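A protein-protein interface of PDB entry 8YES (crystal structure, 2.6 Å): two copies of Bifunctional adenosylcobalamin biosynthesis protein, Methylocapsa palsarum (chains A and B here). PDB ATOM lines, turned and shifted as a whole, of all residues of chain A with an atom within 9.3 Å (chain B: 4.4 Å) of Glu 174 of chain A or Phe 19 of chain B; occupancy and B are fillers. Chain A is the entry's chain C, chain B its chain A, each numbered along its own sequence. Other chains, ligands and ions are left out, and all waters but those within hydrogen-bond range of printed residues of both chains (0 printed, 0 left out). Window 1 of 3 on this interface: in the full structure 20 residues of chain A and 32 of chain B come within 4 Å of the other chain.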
ATOM      1  N   GLN A 149     -30.327  -0.094  -4.778  1.00  0.00           N
ATOM      2  CA  GLN A 149     -29.213   0.895  -4.776  1.00  0.00           C
ATOM      3  C   GLN A 149     -28.648   1.037  -6.199  1.00  0.00           C
ATOM      4  O   GLN A 149     -28.515   2.168  -6.676  1.00  0.00           O
ATOM      5  CB  GLN A 149     -28.127   0.528  -3.768  1.00  0.00           C
ATOM      6  CG  GLN A 149     -28.329   1.157  -2.396  1.00  0.00           C
ATOM      7  CD  GLN A 149     -27.268   0.631  -1.466  1.00  0.00           C
ATOM      8  OE1 GLN A 149     -26.233   1.251  -1.262  1.00  0.00           O
ATOM      9  NE2 GLN A 149     -27.486  -0.560  -0.948  1.00  0.00           N
ATOM     10  N   ALA A 152     -31.481   2.797  -8.585  1.00  0.00           N
ATOM     11  CA  ALA A 152     -31.609   4.218  -8.163  1.00  0.00           C
ATOM     12  C   ALA A 152     -30.428   5.071  -8.691  1.00  0.00           C
ATOM     13  O   ALA A 152     -30.658   6.222  -9.153  1.00  0.00           O
ATOM     14  CB  ALA A 152     -31.694   4.287  -6.664  1.00  0.00           C
ATOM     15  N   GLU A 153     -29.209   4.522  -8.667  1.00  0.00           N
ATOM     16  CA  GLU A 153     -27.984   5.212  -9.138  1.00  0.00           C
ATOM     17  C   GLU A 153     -28.101   5.356 -10.667  1.00  0.00           C
ATOM     18  O   GLU A 153     -28.051   6.489 -11.153  1.00  0.00           O
ATOM     19  CB  GLU A 153     -26.771   4.475  -8.546  1.00  0.00           C
ATOM     20  CG  GLU A 153     -25.473   4.561  -9.323  1.00  0.00           C
ATOM     21  CD  GLU A 153     -24.845   3.181  -9.561  1.00  0.00           C
ATOM     22  OE1 GLU A 153     -23.855   2.856  -8.850  1.00  0.00           O
ATOM     23  OE2 GLU A 153     -25.355   2.404 -10.454  1.00  0.00           O
ATOM     24  N   VAL A 158     -36.166   8.799  -9.545  1.00  0.00           N
ATOM     25  CA  VAL A 158     -36.496   7.786  -8.502  1.00  0.00           C
ATOM     26  C   VAL A 158     -37.628   8.367  -7.652  1.00  0.00           C
ATOM     27  O   VAL A 158     -37.576   9.545  -7.257  1.00  0.00           O
ATOM     28  CB  VAL A 158     -35.273   7.355  -7.661  1.00  0.00           C
ATOM     29  CG1 VAL A 158     -35.612   6.259  -6.667  1.00  0.00           C
ATOM     30  CG2 VAL A 158     -34.101   6.887  -8.513  1.00  0.00           C
ATOM     31  N   ILE A 169     -37.496  11.326  -4.965  1.00  0.00           N
ATOM     32  CA  ILE A 169     -36.226  11.429  -4.198  1.00  0.00           C
ATOM     33  C   ILE A 169     -35.075  11.556  -5.200  1.00  0.00           C
ATOM     34  O   ILE A 169     -33.943  11.533  -4.777  1.00  0.00           O
ATOM     35  CB  ILE A 169     -36.100  10.218  -3.246  1.00  0.00           C
ATOM     36  CG1 ILE A 169     -36.049   8.891  -3.987  1.00  0.00           C
ATOM     37  CG2 ILE A 169     -37.250  10.195  -2.260  1.00  0.00           C
ATOM     38  CD1 ILE A 169     -35.447   7.828  -3.173  1.00  0.00           C
ATOM     39  N   LYS A 170     -35.402  11.651  -6.488  1.00  0.00           N
ATOM     40  CA  LYS A 170     -34.473  11.889  -7.622  1.00  0.00           C
ATOM     41  C   LYS A 170     -35.284  12.252  -8.869  1.00  0.00           C
ATOM     42  O   LYS A 170     -36.350  11.678  -9.097  1.00  0.00           O
ATOM     43  CB  LYS A 170     -33.607  10.662  -7.913  1.00  0.00           C
ATOM     44  CG  LYS A 170     -32.382  10.957  -8.762  1.00  0.00           C
ATOM     45  CD  LYS A 170     -31.483   9.771  -8.944  1.00  0.00           C
ATOM     46  CE  LYS A 170     -30.335  10.065  -9.895  1.00  0.00           C
ATOM     47  NZ  LYS A 170     -29.815   8.832 -10.544  1.00  0.00           N
ATOM     48  N   PRO A 171     -34.807  13.199  -9.722  1.00  0.00           N
ATOM     49  CA  PRO A 171     -33.656  14.039  -9.396  1.00  0.00           C
ATOM     50  C   PRO A 171     -33.932  14.869  -8.137  1.00  0.00           C
ATOM     51  O   PRO A 171     -35.083  14.963  -7.690  1.00  0.00           O
ATOM     52  CB  PRO A 171     -33.480  14.946 -10.623  1.00  0.00           C
ATOM     53  CG  PRO A 171     -34.833  14.897 -11.305  1.00  0.00           C
ATOM     54  CD  PRO A 171     -35.324  13.488 -11.068  1.00  0.00           C
ATOM     55  N   GLY A 172     -32.865  15.439  -7.595  1.00  0.00           N
ATOM     56  CA  GLY A 172     -32.912  16.206  -6.341  1.00  0.00           C
ATOM     57  C   GLY A 172     -31.553  16.124  -5.668  1.00  0.00           C
ATOM     58  O   GLY A 172     -30.913  15.073  -5.662  1.00  0.00           O
ATOM     59  N   PRO A 173     -31.025  17.248  -5.160  1.00  0.00           N
ATOM     60  CA  PRO A 173     -29.723  17.204  -4.490  1.00  0.00           C
ATOM     61  C   PRO A 173     -29.777  16.557  -3.084  1.00  0.00           C
ATOM     62  O   PRO A 173     -30.617  16.893  -2.257  1.00  0.00           O
ATOM     63  CB  PRO A 173     -29.295  18.681  -4.526  1.00  0.00           C
ATOM     64  CG  PRO A 173     -30.598  19.474  -4.611  1.00  0.00           C
ATOM     65  CD  PRO A 173     -31.607  18.589  -5.300  1.00  0.00           C
ATOM     66  N   GLU A 174     -28.889  15.601  -2.833  1.00  0.00           N
ATOM     67  CA  GLU A 174     -28.789  14.938  -1.512  1.00  0.00           C
ATOM     68  C   GLU A 174     -28.280  15.953  -0.487  1.00  0.00           C
ATOM     69  O   GLU A 174     -27.527  16.866  -0.812  1.00  0.00           O
ATOM     70  CB  GLU A 174     -27.889  13.706  -1.602  1.00  0.00           C
ATOM     71  CG  GLU A 174     -28.605  12.469  -2.122  1.00  0.00           C
ATOM     72  CD  GLU A 174     -27.803  11.182  -1.990  1.00  0.00           C
ATOM     73  OE1 GLU A 174     -27.818  10.361  -2.925  1.00  0.00           O
ATOM     74  OE2 GLU A 174     -27.154  10.994  -0.954  1.00  0.00           O
ATOM     75  N   PRO A 175     -28.681  15.830   0.795  1.00  0.00           N
ATOM     76  CA  PRO A 175     -28.188  16.710   1.843  1.00  0.00           C
ATOM     77  C   PRO A 175     -26.701  16.483   2.083  1.00  0.00           C
ATOM     78  O   PRO A 175     -26.229  15.413   1.885  1.00  0.00           O
ATOM     79  CB  PRO A 175     -28.926  16.308   3.117  1.00  0.00           C
ATOM     80  CG  PRO A 175     -30.045  15.405   2.641  1.00  0.00           C
ATOM     81  CD  PRO A 175     -29.603  14.818   1.315  1.00  0.00           C
ATOM     82  N   VAL A 176     -26.011  17.520   2.521  1.00  0.00           N
ATOM     83  CA  VAL A 176     -24.553  17.484   2.841  1.00  0.00           C
ATOM     84  C   VAL A 176     -24.364  18.343   4.096  1.00  0.00           C
ATOM     85  O   VAL A 176     -24.838  19.480   4.102  1.00  0.00           O
ATOM     86  CB  VAL A 176     -23.746  17.977   1.626  1.00  0.00           C
ATOM     87  CG1 VAL A 176     -23.750  19.498   1.540  1.00  0.00           C
ATOM     88  CG2 VAL A 176     -22.337  17.416   1.600  1.00  0.00           C
ATOM     89  N   PHE A 177     -23.793  17.784   5.153  1.00  0.00           N
ATOM     90  CA  PHE A 177     -23.812  18.380   6.515  1.00  0.00           C
ATOM     91  C   PHE A 177     -22.440  18.960   6.876  1.00  0.00           C
ATOM     92  O   PHE A 177     -21.406  18.579   6.316  1.00  0.00           O
ATOM     93  CB  PHE A 177     -24.274  17.325   7.523  1.00  0.00           C
ATOM     94  CG  PHE A 177     -25.721  16.967   7.344  1.00  0.00           C
ATOM     95  CD1 PHE A 177     -26.718  17.847   7.733  1.00  0.00           C
ATOM     96  CD2 PHE A 177     -26.086  15.783   6.724  1.00  0.00           C
ATOM     97  CE1 PHE A 177     -28.055  17.526   7.542  1.00  0.00           C
ATOM     98  CE2 PHE A 177     -27.422  15.472   6.527  1.00  0.00           C
ATOM     99  CZ  PHE A 177     -28.401  16.335   6.939  1.00  0.00           C
ATOM    100  N   PHE A 179     -20.038  19.657  10.060  1.00  0.00           N
ATOM    101  CA  PHE A 179     -19.704  19.264  11.441  1.00  0.00           C
ATOM    102  C   PHE A 179     -18.726  20.293  12.022  1.00  0.00           C
ATOM    103  O   PHE A 179     -18.199  21.126  11.269  1.00  0.00           O
ATOM    104  CB  PHE A 179     -19.175  17.831  11.439  1.00  0.00           C
ATOM    105  CG  PHE A 179     -20.231  16.820  11.092  1.00  0.00           C
ATOM    106  CD1 PHE A 179     -21.312  16.629  11.930  1.00  0.00           C
ATOM    107  CD2 PHE A 179     -20.179  16.119   9.905  1.00  0.00           C
ATOM    108  CE1 PHE A 179     -22.318  15.736  11.605  1.00  0.00           C
ATOM    109  CE2 PHE A 179     -21.171  15.206   9.592  1.00  0.00           C
ATOM    110  CZ  PHE A 179     -22.233  15.011  10.446  1.00  0.00           C
ATOM    111  N   VAL B   8     -28.342   8.823  10.967  1.00  0.00           N
ATOM    112  CA  VAL B   8     -28.695   8.221   9.660  1.00  0.00           C
ATOM    113  C   VAL B   8     -29.493   6.940   9.940  1.00  0.00           C
ATOM    114  O   VAL B   8     -28.882   5.994  10.523  1.00  0.00           O
ATOM    115  CB  VAL B   8     -27.417   7.949   8.852  1.00  0.00           C
ATOM    116  CG1 VAL B   8     -27.702   7.247   7.532  1.00  0.00           C
ATOM    117  CG2 VAL B   8     -26.635   9.226   8.614  1.00  0.00           C
ATOM    118  N   GLY B  15     -27.888   1.569   1.848  1.00  0.00           N
ATOM    119  CA  GLY B  15     -26.796   2.539   1.624  1.00  0.00           C
ATOM    120  C   GLY B  15     -26.531   3.518   2.779  1.00  0.00           C
ATOM    121  O   GLY B  15     -25.840   4.522   2.543  1.00  0.00           O
ATOM    122  N   LYS B  16     -26.988   3.267   4.007  1.00  0.00           N
ATOM    123  CA  LYS B  16     -26.787   4.239   5.120  1.00  0.00           C
ATOM    124  C   LYS B  16     -25.303   4.342   5.542  1.00  0.00           C
ATOM    125  O   LYS B  16     -24.899   5.455   5.879  1.00  0.00           O
ATOM    126  CB  LYS B  16     -27.706   3.915   6.300  1.00  0.00           C
ATOM    127  CG  LYS B  16     -27.548   2.533   6.916  1.00  0.00           C
ATOM    128  CD  LYS B  16     -28.771   2.093   7.730  1.00  0.00           C
ATOM    129  CE  LYS B  16     -28.484   0.903   8.620  1.00  0.00           C
ATOM    130  NZ  LYS B  16     -28.577  -0.385   7.893  1.00  0.00           N
ATOM    131  N   SER B  17     -24.527   3.258   5.558  1.00  0.00           N
ATOM    132  CA  SER B  17     -23.061   3.257   5.829  1.00  0.00           C
ATOM    133  C   SER B  17     -22.278   4.114   4.834  1.00  0.00           C
ATOM    134  O   SER B  17     -21.569   5.032   5.284  1.00  0.00           O
ATOM    135  CB  SER B  17     -22.496   1.887   5.830  1.00  0.00           C
ATOM    136  OG  SER B  17     -22.888   1.236   7.028  1.00  0.00           O
ATOM    137  N   ARG B  18     -22.365   3.785   3.544  1.00  0.00           N
ATOM    138  CA  ARG B  18     -21.837   4.623   2.430  1.00  0.00           C
ATOM    139  C   ARG B  18     -22.118   6.107   2.742  1.00  0.00           C
ATOM    140  O   ARG B  18     -21.196   6.943   2.686  1.00  0.00           O
ATOM    141  CB  ARG B  18     -22.491   4.191   1.115  1.00  0.00           C
ATOM    142  CG  ARG B  18     -21.701   4.510  -0.147  1.00  0.00           C
ATOM    143  CD  ARG B  18     -21.928   3.514  -1.290  1.00  0.00           C
ATOM    144  NE  ARG B  18     -20.659   3.009  -1.822  1.00  0.00           N
ATOM    145  CZ  ARG B  18     -19.843   2.148  -1.194  1.00  0.00           C
ATOM    146  NH1 ARG B  18     -20.147   1.661   0.001  1.00  0.00           N
ATOM    147  NH2 ARG B  18     -18.710   1.780  -1.765  1.00  0.00           N
ATOM    148  N   PHE B  19     -23.343   6.436   3.123  1.00  0.00           N
ATOM    149  CA  PHE B  19     -23.750   7.847   3.297  1.00  0.00           C
ATOM    150  C   PHE B  19     -23.059   8.447   4.523  1.00  0.00           C
ATOM    151  O   PHE B  19     -22.605   9.607   4.457  1.00  0.00           O
ATOM    152  CB  PHE B  19     -25.261   8.015   3.425  1.00  0.00           C
ATOM    153  CG  PHE B  19     -25.644   9.455   3.671  1.00  0.00           C
ATOM    154  CD1 PHE B  19     -25.575  10.382   2.646  1.00  0.00           C
ATOM    155  CD2 PHE B  19     -26.021   9.892   4.929  1.00  0.00           C
ATOM    156  CE1 PHE B  19     -25.921  11.706   2.867  1.00  0.00           C
ATOM    157  CE2 PHE B  19     -26.368  11.215   5.145  1.00  0.00           C
ATOM    158  CZ  PHE B  19     -26.311  12.124   4.119  1.00  0.00           C
ATOM    159  N   ALA B  20     -23.028   7.725   5.632  1.00  0.00           N
ATOM    160  CA  ALA B  20     -22.356   8.201   6.856  1.00  0.00           C
ATOM    161  C   ALA B  20     -20.875   8.387   6.524  1.00  0.00           C
ATOM    162  O   ALA B  20     -20.285   9.402   6.960  1.00  0.00           O
ATOM    163  CB  ALA B  20     -22.565   7.230   7.996  1.00  0.00           C
ATOM    164  N   GLN B  21     -20.302   7.456   5.759  1.00  0.00           N
ATOM    165  CA  GLN B  21     -18.867   7.504   5.398  1.00  0.00           C
ATOM    166  C   GLN B  21     -18.614   8.752   4.528  1.00  0.00           C
ATOM    167  O   GLN B  21     -17.571   9.387   4.698  1.00  0.00           O
ATOM    168  CB  GLN B  21     -18.418   6.212   4.722  1.00  0.00           C
ATOM    169  CG  GLN B  21     -16.967   6.258   4.276  1.00  0.00           C
ATOM    170  CD  GLN B  21     -16.448   4.923   3.825  1.00  0.00           C
ATOM    171  OE1 GLN B  21     -17.069   3.881   4.022  1.00  0.00           O
ATOM    172  NE2 GLN B  21     -15.288   4.943   3.203  1.00  0.00           N
ATOM    173  N   ARG B  22     -19.542   9.127   3.653  1.00  0.00           N
ATOM    174  CA  ARG B  22     -19.325  10.282   2.743  1.00  0.00           C
ATOM    175  C   ARG B  22     -19.350  11.592   3.541  1.00  0.00           C
ATOM    176  O   ARG B  22     -18.463  12.402   3.325  1.00  0.00           O
ATOM    177  CB  ARG B  22     -20.364  10.312   1.624  1.00  0.00           C
ATOM    178  CG  ARG B  22     -19.798  10.757   0.295  1.00  0.00           C
ATOM    179  CD  ARG B  22     -20.784  10.426  -0.789  1.00  0.00           C
ATOM    180  NE  ARG B  22     -22.041  11.148  -0.616  1.00  0.00           N
ATOM    181  CZ  ARG B  22     -23.237  10.612  -0.832  1.00  0.00           C
ATOM    182  NH1 ARG B  22     -23.349   9.328  -1.135  1.00  0.00           N
ATOM    183  NH2 ARG B  22     -24.323  11.353  -0.709  1.00  0.00           N
ATOM    184  N   MET B  23     -20.330  11.786   4.412  1.00  0.00           N
ATOM    185  CA  MET B  23     -20.444  12.983   5.287  1.00  0.00           C
ATOM    186  C   MET B  23     -19.223  13.063   6.219  1.00  0.00           C
ATOM    187  O   MET B  23     -18.786  14.187   6.525  1.00  0.00           O
ATOM    188  CB  MET B  23     -21.718  12.943   6.139  1.00  0.00           C
ATOM    189  CG  MET B  23     -23.017  12.939   5.345  1.00  0.00           C
ATOM    190  SD  MET B  23     -23.207  14.359   4.221  1.00  0.00           S
ATOM    191  CE  MET B  23     -22.627  13.610   2.698  1.00  0.00           C
ATOM    192  N   THR B 159     -31.304  12.227   8.931  1.00  0.00           N
ATOM    193  CA  THR B 159     -31.472  11.871   7.501  1.00  0.00           C
ATOM    194  C   THR B 159     -32.051  10.443   7.390  1.00  0.00           C
ATOM    195  O   THR B 159     -31.682   9.561   8.191  1.00  0.00           O
ATOM    196  CB  THR B 159     -30.145  12.140   6.792  1.00  0.00           C
ATOM    197  OG1 THR B 159     -30.411  12.087   5.393  1.00  0.00           O
ATOM    198  CG2 THR B 159     -29.082  11.138   7.173  1.00  0.00           C
ATOM    199  N   VAL B 161     -32.471   7.272   4.682  1.00  0.00           N
ATOM    200  CA  VAL B 161     -31.817   6.756   3.446  1.00  0.00           C
ATOM    201  C   VAL B 161     -32.644   5.596   2.855  1.00  0.00           C
ATOM    202  O   VAL B 161     -32.858   4.590   3.554  1.00  0.00           O
ATOM    203  CB  VAL B 161     -30.373   6.315   3.733  1.00  0.00           C
ATOM    204  CG1 VAL B 161     -29.651   5.848   2.465  1.00  0.00           C
ATOM    205  CG2 VAL B 161     -29.585   7.425   4.410  1.00  0.00           C
ATOM    206  N   GLY B 164     -30.128   3.901  -1.485  1.00  0.00           N
ATOM    207  CA  GLY B 164     -28.813   4.584  -1.597  1.00  0.00           C
ATOM    208  C   GLY B 164     -28.925   6.098  -1.586  1.00  0.00           C
ATOM    209  O   GLY B 164     -27.910   6.747  -1.819  1.00  0.00           O
ATOM    210  N   ILE B 165     -30.108   6.639  -1.312  1.00  0.00           N
ATOM    211  CA  ILE B 165     -30.405   8.091  -1.436  1.00  0.00           C
ATOM    212  C   ILE B 165     -30.905   8.644  -0.102  1.00  0.00           C
ATOM    213  O   ILE B 165     -31.841   8.078   0.468  1.00  0.00           O
ATOM    214  CB  ILE B 165     -31.425   8.341  -2.557  1.00  0.00           C
ATOM    215  CG1 ILE B 165     -30.810   8.026  -3.921  1.00  0.00           C
ATOM    216  CG2 ILE B 165     -31.950   9.765  -2.496  1.00  0.00           C
ATOM    217  CD1 ILE B 165     -31.822   7.931  -5.050  1.00  0.00           C
ATOM    218  N   ALA B 166     -30.321   9.764   0.328  1.00  0.00           N
ATOM    219  CA  ALA B 166     -30.597  10.419   1.620  1.00  0.00           C
ATOM    220  C   ALA B 166     -31.632  11.522   1.429  1.00  0.00           C
ATOM    221  O   ALA B 166     -31.608  12.254   0.389  1.00  0.00           O
ATOM    222  CB  ALA B 166     -29.320  10.956   2.198  1.00  0.00           C
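Among the printed residues, pairs that only touch across the chains: Gln 149 of chain A with Gly 15 of chain B (3.2 Å), Gln 149 of chain A with Gly 164 of chain B (3.4 Å), Ala 152 of chain A with Ile 165 of chain B (3.99 Å), Ile 169 of chain A with Ile 165 of chain B (3.5 Å), Glu 174 of chain A with Phe 19 of chain B (3.98 Å), Glu 174 of chain A with Gly 164 of chain B (3.8 Å), Glu 174 of chain A with Ile 165 of chain B (3.8 Å), Glu 174 of chain A with Ala 166 of chain B (3.6 Å), Pro 175 of chain A with Phe 19 of chain B (3.8 Å), Pro 175 of chain A with Met 23 of chain B (3.96 Å), Pro 175 of chain A with Ala 166 of chain B (3.4 Å) and Val 176 of chain A with Met 23 of chain B (3.7 Å).
Of the printed residues of chain B, Gln 149 of chain A touches Gly 15 (3.2 Å) and Gly 164 (3.4 Å). Of the printed residues of chain B, Ala 152 of chain A touches Ile 165 (3.99 Å). Gly 172 of chain A touches none of the printed residues of chain B. Glu 174 of chain A touches five residues of chain B. Phe 19 of chain B touches just these residues of chain A: Glu 174 and Pro 175. Thr 159 of chain B touches none of the printed residues of chain A. Printed residues of chain A within 4 Å of Gly 164 of chain B: Gln 149 (3.4 Å) and Glu 174 (3.8 Å). Ala 166 of chain B touches just these residues of chain A: Glu 174 (3.6 Å) and Pro 175 (3.4 Å). The nearest printed residue of chain B that does not touch Glu 174 of chain A is Met 23 of chain B (6.4 Å). The nearest residue of chain A that does not touch Phe 19 of chain B is Phe 177 of chain A (4.3 Å). The nearest printed residue of chain B that does not touch Gln 149 of chain A is Arg 18 of chain B (4.9 Å).
Of the 14 printed residues of chain A, 7 touch a printed residue of chain B. Printed residues of chain A that touch a printed residue of chain B: Gln 149, Ala 152, Ile 169, Glu 174, Pro 175, Val 176 and Phe 177. Hydrophobic or aromatic side chains of chain A that line the printed part of chain B: Ala 152, Pro 175 and Val 176. Hydrophobic or aromatic side chains of chain B that line the printed part of chain A: Phe 19, Met 23, Ile 165 and Ala 166. Among the printed residues, 14 pairs touch across the chains.
The backbone carbonyl oxygen (O) of Ala 152 of chain A is in hydrogen-bond range of the side-chain amino group (NZ) of Lys 170 of chain A (3.1 Å). The backbone carbonyl oxygen (O) of Val 158 of chain A lies within hydrogen-bond range of the backbone NH (N) of Ile 169 of chain A (2.9 Å).
No position is printed for both chains. Of the 14 pairs that touch across the chains among the printed residues, none has its exchanged pair printed and touching as well.
The guanidinium group (NH2) of Arg 22 of chain B lies within salt-bridge range of the side-chain carboxylate (OE2) of Glu 174 of chain A, 2.9 Å away. The backbone NH of Phe 177 of chain A is in hydrogen-bond range of the side-chain sulfur of Met 23 of chain B.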
